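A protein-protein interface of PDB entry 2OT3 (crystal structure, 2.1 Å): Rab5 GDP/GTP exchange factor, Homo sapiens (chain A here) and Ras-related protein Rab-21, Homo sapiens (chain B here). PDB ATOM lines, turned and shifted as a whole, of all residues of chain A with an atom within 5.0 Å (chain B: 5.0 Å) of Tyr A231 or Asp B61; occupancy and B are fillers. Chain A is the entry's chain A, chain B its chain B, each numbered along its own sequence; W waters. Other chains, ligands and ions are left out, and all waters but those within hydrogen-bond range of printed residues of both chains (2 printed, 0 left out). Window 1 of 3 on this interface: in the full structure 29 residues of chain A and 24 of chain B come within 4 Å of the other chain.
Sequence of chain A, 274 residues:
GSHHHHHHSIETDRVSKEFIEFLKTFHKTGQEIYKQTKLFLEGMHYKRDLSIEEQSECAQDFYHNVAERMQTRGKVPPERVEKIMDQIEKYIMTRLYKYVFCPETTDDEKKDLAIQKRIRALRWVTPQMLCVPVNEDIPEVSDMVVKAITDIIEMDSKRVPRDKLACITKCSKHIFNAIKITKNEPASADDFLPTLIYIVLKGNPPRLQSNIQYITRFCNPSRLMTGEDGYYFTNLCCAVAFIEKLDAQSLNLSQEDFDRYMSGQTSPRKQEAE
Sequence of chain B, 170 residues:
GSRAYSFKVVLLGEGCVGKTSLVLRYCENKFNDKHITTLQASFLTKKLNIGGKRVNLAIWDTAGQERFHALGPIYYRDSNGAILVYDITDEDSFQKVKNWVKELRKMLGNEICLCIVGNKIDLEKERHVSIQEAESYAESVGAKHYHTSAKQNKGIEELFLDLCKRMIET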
ATOM      1  N   SER A 188      -4.675 -17.651   4.640  1.00  0.00           N
ATOM      2  CA  SER A 188      -4.563 -18.832   5.498  1.00  0.00           C
ATOM      3  C   SER A 188      -3.877 -18.419   6.831  1.00  0.00           C
ATOM      4  O   SER A 188      -3.411 -17.278   6.974  1.00  0.00           O
ATOM      5  CB  SER A 188      -3.706 -19.855   4.771  1.00  0.00           C
ATOM      6  OG  SER A 188      -2.391 -19.354   4.690  1.00  0.00           O
ATOM      7  N   ALA A 189      -3.775 -19.341   7.791  1.00  0.00           N
ATOM      8  CA  ALA A 189      -3.025 -19.046   9.023  1.00  0.00           C
ATOM      9  C   ALA A 189      -1.589 -18.679   8.697  1.00  0.00           C
ATOM     10  O   ALA A 189      -1.005 -17.798   9.339  1.00  0.00           O
ATOM     11  CB  ALA A 189      -3.059 -20.203   9.991  1.00  0.00           C
ATOM     12  N   ASP A 190      -1.031 -19.330   7.680  1.00  0.00           N
ATOM     13  CA  ASP A 190       0.348 -19.040   7.248  1.00  0.00           C
ATOM     14  C   ASP A 190       0.524 -17.585   6.769  1.00  0.00           C
ATOM     15  O   ASP A 190       1.565 -16.986   6.980  1.00  0.00           O
ATOM     16  CB  ASP A 190       0.822 -20.044   6.187  1.00  0.00           C
ATOM     17  CG  ASP A 190       0.533 -21.515   6.582  1.00  0.00           C
ATOM     18  OD1 ASP A 190       1.492 -22.263   6.761  1.00  0.00           O
ATOM     19  OD2 ASP A 190      -0.645 -21.925   6.727  1.00  0.00           O
ATOM     20  N   PHE A 192      -1.711 -15.118   7.796  1.00  0.00           N
ATOM     21  CA  PHE A 192      -2.303 -14.253   8.821  1.00  0.00           C
ATOM     22  C   PHE A 192      -1.350 -14.008   9.986  1.00  0.00           C
ATOM     23  O   PHE A 192      -1.132 -12.866  10.392  1.00  0.00           O
ATOM     24  CB  PHE A 192      -3.647 -14.828   9.329  1.00  0.00           C
ATOM     25  CG  PHE A 192      -4.264 -14.032  10.492  1.00  0.00           C
ATOM     26  CD1 PHE A 192      -4.671 -12.701  10.315  1.00  0.00           C
ATOM     27  CD2 PHE A 192      -4.446 -14.615  11.729  1.00  0.00           C
ATOM     28  CE1 PHE A 192      -5.229 -11.966  11.363  1.00  0.00           C
ATOM     29  CE2 PHE A 192      -4.998 -13.880  12.805  1.00  0.00           C
ATOM     30  CZ  PHE A 192      -5.387 -12.548  12.609  1.00  0.00           C
ATOM     31  N   GLY A 227     -15.491 -19.777  18.950  1.00  0.00           N
ATOM     32  CA  GLY A 227     -15.958 -18.674  18.061  1.00  0.00           C
ATOM     33  C   GLY A 227     -14.820 -17.778  17.612  1.00  0.00           C
ATOM     34  O   GLY A 227     -13.692 -17.967  18.047  1.00  0.00           O
ATOM     35  N   GLU A 228     -15.098 -16.797  16.742  1.00  0.00           N
ATOM     36  CA  GLU A 228     -14.009 -16.046  16.097  1.00  0.00           C
ATOM     37  C   GLU A 228     -13.153 -15.232  17.073  1.00  0.00           C
ATOM     38  O   GLU A 228     -11.939 -15.142  16.890  1.00  0.00           O
ATOM     39  CB  GLU A 228     -14.501 -15.195  14.918  1.00  0.00           C
ATOM     40  CG  GLU A 228     -15.323 -13.971  15.331  1.00  0.00           C
ATOM     41  CD  GLU A 228     -15.677 -13.046  14.176  1.00  0.00           C
ATOM     42  OE1 GLU A 228     -15.250 -13.299  13.031  1.00  0.00           O
ATOM     43  OE2 GLU A 228     -16.365 -12.041  14.437  1.00  0.00           O
ATOM     44  N   ASP A 229     -13.760 -14.665  18.118  1.00  0.00           N
ATOM     45  CA  ASP A 229     -12.985 -13.894  19.102  1.00  0.00           C
ATOM     46  C   ASP A 229     -11.905 -14.770  19.745  1.00  0.00           C
ATOM     47  O   ASP A 229     -10.803 -14.302  20.020  1.00  0.00           O
ATOM     48  CB  ASP A 229     -13.885 -13.300  20.198  1.00  0.00           C
ATOM     49  CG  ASP A 229     -14.704 -12.102  19.725  1.00  0.00           C
ATOM     50  OD1 ASP A 229     -14.583 -11.669  18.556  1.00  0.00           O
ATOM     51  OD2 ASP A 229     -15.463 -11.562  20.565  1.00  0.00           O
ATOM     52  N   GLY A 230     -12.245 -16.034  20.001  1.00  0.00           N
ATOM     53  CA  GLY A 230     -11.290 -17.000  20.547  1.00  0.00           C
ATOM     54  C   GLY A 230     -10.127 -17.274  19.612  1.00  0.00           C
ATOM     55  O   GLY A 230      -8.978 -17.338  20.062  1.00  0.00           O
ATOM     56  N   TYR A 231     -10.428 -17.455  18.318  1.00  0.00           N
ATOM     57  CA  TYR A 231      -9.401 -17.655  17.295  1.00  0.00           C
ATOM     58  C   TYR A 231      -8.406 -16.488  17.231  1.00  0.00           C
ATOM     59  O   TYR A 231      -7.193 -16.698  17.248  1.00  0.00           O
ATOM     60  CB  TYR A 231     -10.008 -17.896  15.900  1.00  0.00           C
ATOM     61  CG  TYR A 231      -8.940 -18.238  14.850  1.00  0.00           C
ATOM     62  CD1 TYR A 231      -8.319 -19.498  14.840  1.00  0.00           C
ATOM     63  CD2 TYR A 231      -8.561 -17.305  13.863  1.00  0.00           C
ATOM     64  CE1 TYR A 231      -7.329 -19.807  13.886  1.00  0.00           C
ATOM     65  CE2 TYR A 231      -7.564 -17.602  12.919  1.00  0.00           C
ATOM     66  CZ  TYR A 231      -6.964 -18.866  12.947  1.00  0.00           C
ATOM     67  OH  TYR A 231      -6.012 -19.187  12.008  1.00  0.00           O
ATOM     68  N   TYR A 232      -8.922 -15.264  17.135  1.00  0.00           N
ATOM     69  CA  TYR A 232      -8.065 -14.080  17.036  1.00  0.00           C
ATOM     70  C   TYR A 232      -7.276 -13.832  18.304  1.00  0.00           C
ATOM     71  O   TYR A 232      -6.101 -13.466  18.222  1.00  0.00           O
ATOM     72  CB  TYR A 232      -8.880 -12.850  16.577  1.00  0.00           C
ATOM     73  CG  TYR A 232      -9.574 -13.175  15.286  1.00  0.00           C
ATOM     74  CD1 TYR A 232      -8.852 -13.710  14.224  1.00  0.00           C
ATOM     75  CD2 TYR A 232     -10.951 -13.000  15.128  1.00  0.00           C
ATOM     76  CE1 TYR A 232      -9.464 -14.041  13.031  1.00  0.00           C
ATOM     77  CE2 TYR A 232     -11.576 -13.333  13.927  1.00  0.00           C
ATOM     78  CZ  TYR A 232     -10.818 -13.868  12.891  1.00  0.00           C
ATOM     79  OH  TYR A 232     -11.402 -14.243  11.685  1.00  0.00           O
ATOM     80  N   PHE A 233      -7.890 -14.084  19.465  1.00  0.00           N
ATOM     81  CA  PHE A 233      -7.177 -13.960  20.725  1.00  0.00           C
ATOM     82  C   PHE A 233      -6.025 -14.979  20.794  1.00  0.00           C
ATOM     83  O   PHE A 233      -4.893 -14.640  21.147  1.00  0.00           O
ATOM     84  CB  PHE A 233      -8.123 -14.140  21.927  1.00  0.00           C
ATOM     85  CG  PHE A 233      -7.403 -14.125  23.245  1.00  0.00           C
ATOM     86  CD1 PHE A 233      -6.802 -12.954  23.704  1.00  0.00           C
ATOM     87  CD2 PHE A 233      -7.274 -15.290  24.001  1.00  0.00           C
ATOM     88  CE1 PHE A 233      -6.102 -12.947  24.908  1.00  0.00           C
ATOM     89  CE2 PHE A 233      -6.581 -15.293  25.222  1.00  0.00           C
ATOM     90  CZ  PHE A 233      -5.995 -14.119  25.667  1.00  0.00           C
ATOM     91  N   THR A 234      -6.321 -16.229  20.443  1.00  0.00           N
ATOM     92  CA  THR A 234      -5.286 -17.266  20.353  1.00  0.00           C
ATOM     93  C   THR A 234      -4.156 -16.841  19.441  1.00  0.00           C
ATOM     94  O   THR A 234      -2.994 -17.048  19.771  1.00  0.00           O
ATOM     95  CB  THR A 234      -5.883 -18.581  19.844  1.00  0.00           C
ATOM     96  OG1 THR A 234      -6.715 -19.126  20.887  1.00  0.00           O
ATOM     97  CG2 THR A 234      -4.775 -19.581  19.448  1.00  0.00           C
ATOM     98  N   ASN A 235      -4.491 -16.230  18.309  1.00  0.00           N
ATOM     99  CA  ASN A 235      -3.469 -15.750  17.389  1.00  0.00           C
ATOM    100  C   ASN A 235      -2.626 -14.653  17.993  1.00  0.00           C
ATOM    101  O   ASN A 235      -1.409 -14.645  17.804  1.00  0.00           O
ATOM    102  CB  ASN A 235      -4.051 -15.312  16.035  1.00  0.00           C
ATOM    103  CG  ASN A 235      -4.136 -16.475  15.073  1.00  0.00           C
ATOM    104  OD1 ASN A 235      -3.187 -16.746  14.362  1.00  0.00           O
ATOM    105  ND2 ASN A 235      -5.237 -17.233  15.126  1.00  0.00           N
ATOM    106  N   LEU B  11      -6.764 -27.232  11.998  1.00  0.00           N
ATOM    107  CA  LEU B  11      -6.318 -27.645  10.671  1.00  0.00           C
ATOM    108  C   LEU B  11      -4.790 -27.514  10.568  1.00  0.00           C
ATOM    109  O   LEU B  11      -4.239 -26.436  10.791  1.00  0.00           O
ATOM    110  CB  LEU B  11      -7.024 -26.801   9.586  1.00  0.00           C
ATOM    111  CG  LEU B  11      -6.658 -26.999   8.100  1.00  0.00           C
ATOM    112  CD1 LEU B  11      -7.067 -28.392   7.601  1.00  0.00           C
ATOM    113  CD2 LEU B  11      -7.321 -25.955   7.261  1.00  0.00           C
ATOM    114  N   LYS B  19      -4.261 -27.608   1.954  1.00  0.00           N
ATOM    115  CA  LYS B  19      -5.235 -27.559   3.055  1.00  0.00           C
ATOM    116  C   LYS B  19      -6.309 -26.471   2.890  1.00  0.00           C
ATOM    117  O   LYS B  19      -7.459 -26.647   3.331  1.00  0.00           O
ATOM    118  CB  LYS B  19      -4.540 -27.344   4.408  1.00  0.00           C
ATOM    119  CG  LYS B  19      -3.804 -26.011   4.544  1.00  0.00           C
ATOM    120  CD  LYS B  19      -3.498 -25.682   6.018  1.00  0.00           C
ATOM    121  CE  LYS B  19      -2.630 -24.450   6.108  1.00  0.00           C
ATOM    122  NZ  LYS B  19      -2.172 -24.240   7.491  1.00  0.00           N
ATOM    123  N   THR B  20      -5.925 -25.343   2.304  1.00  0.00           N
ATOM    124  CA  THR B  20      -6.845 -24.216   2.215  1.00  0.00           C
ATOM    125  C   THR B  20      -7.938 -24.481   1.180  1.00  0.00           C
ATOM    126  O   THR B  20      -9.107 -24.204   1.430  1.00  0.00           O
ATOM    127  CB  THR B  20      -6.122 -22.883   1.908  1.00  0.00           C
ATOM    128  OG1 THR B  20      -5.268 -22.541   3.007  1.00  0.00           O
ATOM    129  CG2 THR B  20      -7.134 -21.774   1.755  1.00  0.00           C
ATOM    130  N   ALA B  41      -9.504 -17.320   5.084  1.00  0.00           N
ATOM    131  CA  ALA B  41      -9.651 -18.758   5.153  1.00  0.00           C
ATOM    132  C   ALA B  41      -8.949 -19.333   6.375  1.00  0.00           C
ATOM    133  O   ALA B  41      -8.500 -20.484   6.343  1.00  0.00           O
ATOM    134  CB  ALA B  41      -9.150 -19.411   3.840  1.00  0.00           C
ATOM    135  N   SER B  42      -8.866 -18.538   7.454  1.00  0.00           N
ATOM    136  CA  SER B  42      -8.140 -18.935   8.656  1.00  0.00           C
ATOM    137  C   SER B  42      -9.075 -19.453   9.739  1.00  0.00           C
ATOM    138  O   SER B  42      -8.735 -20.370  10.471  1.00  0.00           O
ATOM    139  CB  SER B  42      -7.296 -17.782   9.201  1.00  0.00           C
ATOM    140  OG  SER B  42      -6.381 -17.327   8.238  1.00  0.00           O
ATOM    141  N   PHE B  43     -10.254 -18.841   9.825  1.00  0.00           N
ATOM    142  CA  PHE B  43     -11.281 -19.253  10.746  1.00  0.00           C
ATOM    143  C   PHE B  43     -12.583 -19.463   9.969  1.00  0.00           C
ATOM    144  O   PHE B  43     -13.117 -18.542   9.351  1.00  0.00           O
ATOM    145  CB  PHE B  43     -11.503 -18.202  11.832  1.00  0.00           C
ATOM    146  CG  PHE B  43     -12.621 -18.554  12.773  1.00  0.00           C
ATOM    147  CD1 PHE B  43     -12.415 -19.474  13.791  1.00  0.00           C
ATOM    148  CD2 PHE B  43     -13.892 -18.029  12.589  1.00  0.00           C
ATOM    149  CE1 PHE B  43     -13.452 -19.820  14.654  1.00  0.00           C
ATOM    150  CE2 PHE B  43     -14.938 -18.378  13.434  1.00  0.00           C
ATOM    151  CZ  PHE B  43     -14.717 -19.258  14.474  1.00  0.00           C
ATOM    152  N   ILE B  59     -13.546 -24.339  12.308  1.00  0.00           N
ATOM    153  CA  ILE B  59     -12.272 -24.764  11.784  1.00  0.00           C
ATOM    154  C   ILE B  59     -11.219 -23.696  12.060  1.00  0.00           C
ATOM    155  O   ILE B  59     -11.311 -22.592  11.527  1.00  0.00           O
ATOM    156  CB  ILE B  59     -12.308 -25.034  10.248  1.00  0.00           C
ATOM    157  CG1 ILE B  59     -13.538 -25.857   9.830  1.00  0.00           C
ATOM    158  CG2 ILE B  59     -11.010 -25.716   9.820  1.00  0.00           C
ATOM    159  CD1 ILE B  59     -13.528 -27.231  10.329  1.00  0.00           C
ATOM    160  N   TRP B  60     -10.221 -24.035  12.867  1.00  0.00           N
ATOM    161  CA  TRP B  60      -9.152 -23.101  13.227  1.00  0.00           C
ATOM    162  C   TRP B  60      -7.904 -23.453  12.444  1.00  0.00           C
ATOM    163  O   TRP B  60      -7.225 -24.425  12.782  1.00  0.00           O
ATOM    164  CB  TRP B  60      -8.804 -23.228  14.704  1.00  0.00           C
ATOM    165  CG  TRP B  60      -9.826 -22.720  15.657  1.00  0.00           C
ATOM    166  CD1 TRP B  60     -11.194 -22.801  15.534  1.00  0.00           C
ATOM    167  CD2 TRP B  60      -9.573 -22.072  16.899  1.00  0.00           C
ATOM    168  NE1 TRP B  60     -11.793 -22.226  16.623  1.00  0.00           N
ATOM    169  CE2 TRP B  60     -10.820 -21.766  17.473  1.00  0.00           C
ATOM    170  CE3 TRP B  60      -8.411 -21.702  17.575  1.00  0.00           C
ATOM    171  CZ2 TRP B  60     -10.937 -21.109  18.691  1.00  0.00           C
ATOM    172  CZ3 TRP B  60      -8.533 -21.051  18.786  1.00  0.00           C
ATOM    173  CH2 TRP B  60      -9.783 -20.761  19.331  1.00  0.00           C
ATOM    174  N   ASP B  61      -7.594 -22.690  11.399  1.00  0.00           N
ATOM    175  CA  ASP B  61      -6.333 -22.927  10.690  1.00  0.00           C
ATOM    176  C   ASP B  61      -5.120 -22.610  11.570  1.00  0.00           C
ATOM    177  O   ASP B  61      -5.115 -21.616  12.293  1.00  0.00           O
ATOM    178  CB  ASP B  61      -6.257 -22.152   9.367  1.00  0.00           C
ATOM    179  CG  ASP B  61      -5.163 -22.687   8.437  1.00  0.00           C
ATOM    180  OD1 ASP B  61      -4.658 -23.826   8.647  1.00  0.00           O
ATOM    181  OD2 ASP B  61      -4.792 -21.970   7.504  1.00  0.00           O
ATOM    182  N   THR B  62      -4.084 -23.455  11.507  1.00  0.00           N
ATOM    183  CA  THR B  62      -2.859 -23.191  12.269  1.00  0.00           C
ATOM    184  C   THR B  62      -1.644 -23.009  11.319  1.00  0.00           C
ATOM    185  O   THR B  62      -1.544 -23.679  10.307  1.00  0.00           O
ATOM    186  CB  THR B  62      -2.606 -24.310  13.342  1.00  0.00           C
ATOM    187  OG1 THR B  62      -2.259 -25.537  12.693  1.00  0.00           O
ATOM    188  CG2 THR B  62      -3.868 -24.550  14.188  1.00  0.00           C
ATOM    189  N   ALA B  63      -0.762 -22.068  11.633  1.00  0.00           N
ATOM    190  CA  ALA B  63       0.362 -21.718  10.752  1.00  0.00           C
ATOM    191  C   ALA B  63       1.321 -22.908  10.665  1.00  0.00           C
ATOM    192  O   ALA B  63       1.830 -23.350  11.693  1.00  0.00           O
ATOM    193  CB  ALA B  63       1.103 -20.503  11.285  1.00  0.00           C
ATOM    194  N   TYR B  75      -2.352 -22.920  19.806  1.00  0.00           N
ATOM    195  CA  TYR B  75      -3.491 -23.204  18.946  1.00  0.00           C
ATOM    196  C   TYR B  75      -4.306 -24.446  19.361  1.00  0.00           C
ATOM    197  O   TYR B  75      -5.548 -24.442  19.302  1.00  0.00           O
ATOM    198  CB  TYR B  75      -2.998 -23.530  17.558  1.00  0.00           C
ATOM    199  CG  TYR B  75      -2.588 -22.418  16.623  1.00  0.00           C
ATOM    200  CD1 TYR B  75      -3.531 -21.523  16.115  1.00  0.00           C
ATOM    201  CD2 TYR B  75      -1.266 -22.353  16.145  1.00  0.00           C
ATOM    202  CE1 TYR B  75      -3.153 -20.532  15.187  1.00  0.00           C
ATOM    203  CE2 TYR B  75      -0.876 -21.388  15.220  1.00  0.00           C
ATOM    204  CZ  TYR B  75      -1.831 -20.484  14.736  1.00  0.00           C
ATOM    205  OH  TYR B  75      -1.462 -19.543  13.811  1.00  0.00           O
HETATM  206  O   HOH W   1      -3.076 -18.259  12.422  1.00  0.00           O
HETATM  207  O   HOH W   2      -6.281 -21.917  21.600  1.00  0.00           O
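Among the printed residues, pairs that only touch across the chains: Ser A188 with Thr B20, Ser A188 with Asp B61, Ala A189 with Thr B62, Ala A189 with Ala B63, Asp A190 with Ala B63, Phe A192 with Ser B42, Gly A227 with Phe B43, Glu A228 with Phe B43, Gly A230 with Trp B60, Tyr A231 with Phe B43, Tyr A231 with Trp B60, Tyr A232 with Phe B43, Thr A234 with Trp B60 and Thr A234 with Tyr B75.
Of the 12 printed residues of chain B, 9 touch a printed residue of chain A.
Among the printed residues, Asp or Glu carboxylates within 4 Å of a Lys or Arg side-chain nitrogen of the other chain: Asp A190 with Lys B19 (2.9 Å).
Water W1 lies within hydrogen-bond range of the side-chain amide oxygen (OD1) of Asn A235 (2.5 Å), the side-chain hydroxyl (OH) of Tyr B75 (2.5 Å) and the side-chain hydroxyl (OH) of Tyr A231 (3.1 Å).
Water W2 bridges OG1 of Thr A234 (2.9 Å) and O of Tyr B75 (3.5 Å).
OG of Ser B42 sits close to O of Ser A188 (3.2 Å).
The backbone NH of Ala A189 lies within hydrogen-bond range of the side-chain hydroxyl of Ser B42.
OD2 of Asp B61 lies within hydrogen-bond range of N of Ala A189 (2.8 Å).
OD2 of Asp A190 lies within salt-bridge range of NZ of Lys B19, 2.9 Å away.
The backbone carbonyl oxygen of Ser B42 lies within hydrogen-bond range of the side-chain hydroxyl of Tyr A231.
The backbone carbonyl oxygen of Asp B61 lies within hydrogen-bond range of the side-chain hydroxyl of Tyr A231, at 2.6 Å.
OH of Tyr B75 is in hydrogen-bond range of OD1 of Asn A235 (3.3 Å).
The side-chain hydroxyl (OG) of Ser A188 lies close to the backbone NH (N) of Asp A190, 3.3 Å away.
The backbone carbonyl oxygen of Gly A230 lies within hydrogen-bond range of the side-chain hydroxyl of Thr A234.
O of Tyr A231 lies within hydrogen-bond range of ND2 of Asn A235 (2.9 Å).
The backbone carbonyl oxygen (O) of Leu B11 lies within hydrogen-bond range of the side-chain hydroxyl (OG1) of Thr B62 (2.9 Å).
The side-chain amino group (NZ) of Lys B19 lies within salt-bridge range of the side-chain carboxylate (OD1) of Asp B61.
The side-chain hydroxyl (OH) of Tyr B75 sits at hydrogen-bond distance from the backbone NH (N) of Ala B63, 3.4 Å away.
Of the printed residues of chain B, Asp A190 touches Lys B19 and Ala B63.
Tyr A231 touches four residues of chain B.
Of the printed residues of chain B, Tyr A232 touches Phe B43 (3.96 Å).
Asp B61 touches just these residues of chain A: Ser A188 (3.6 Å), Ala A189 (2.8 Å) and Tyr A231 (2.6 Å).
Printed residues of chain A within 4 Å of Thr B62: Ala A189 (3.4 Å).
Of the printed residues of chain A, Ala B63 touches Ala A189 and Asp A190.
Of the printed residues of chain A, Tyr B75 touches Thr A234 (3.9 Å) and Asn A235 (3.3 Å).
The nearest residue of chain A that does not touch Asp B61 is Asp A190 (4.2 Å).
The nearest printed residue of chain A that does not touch Trp B60 is Gly A227 (4.2 Å).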
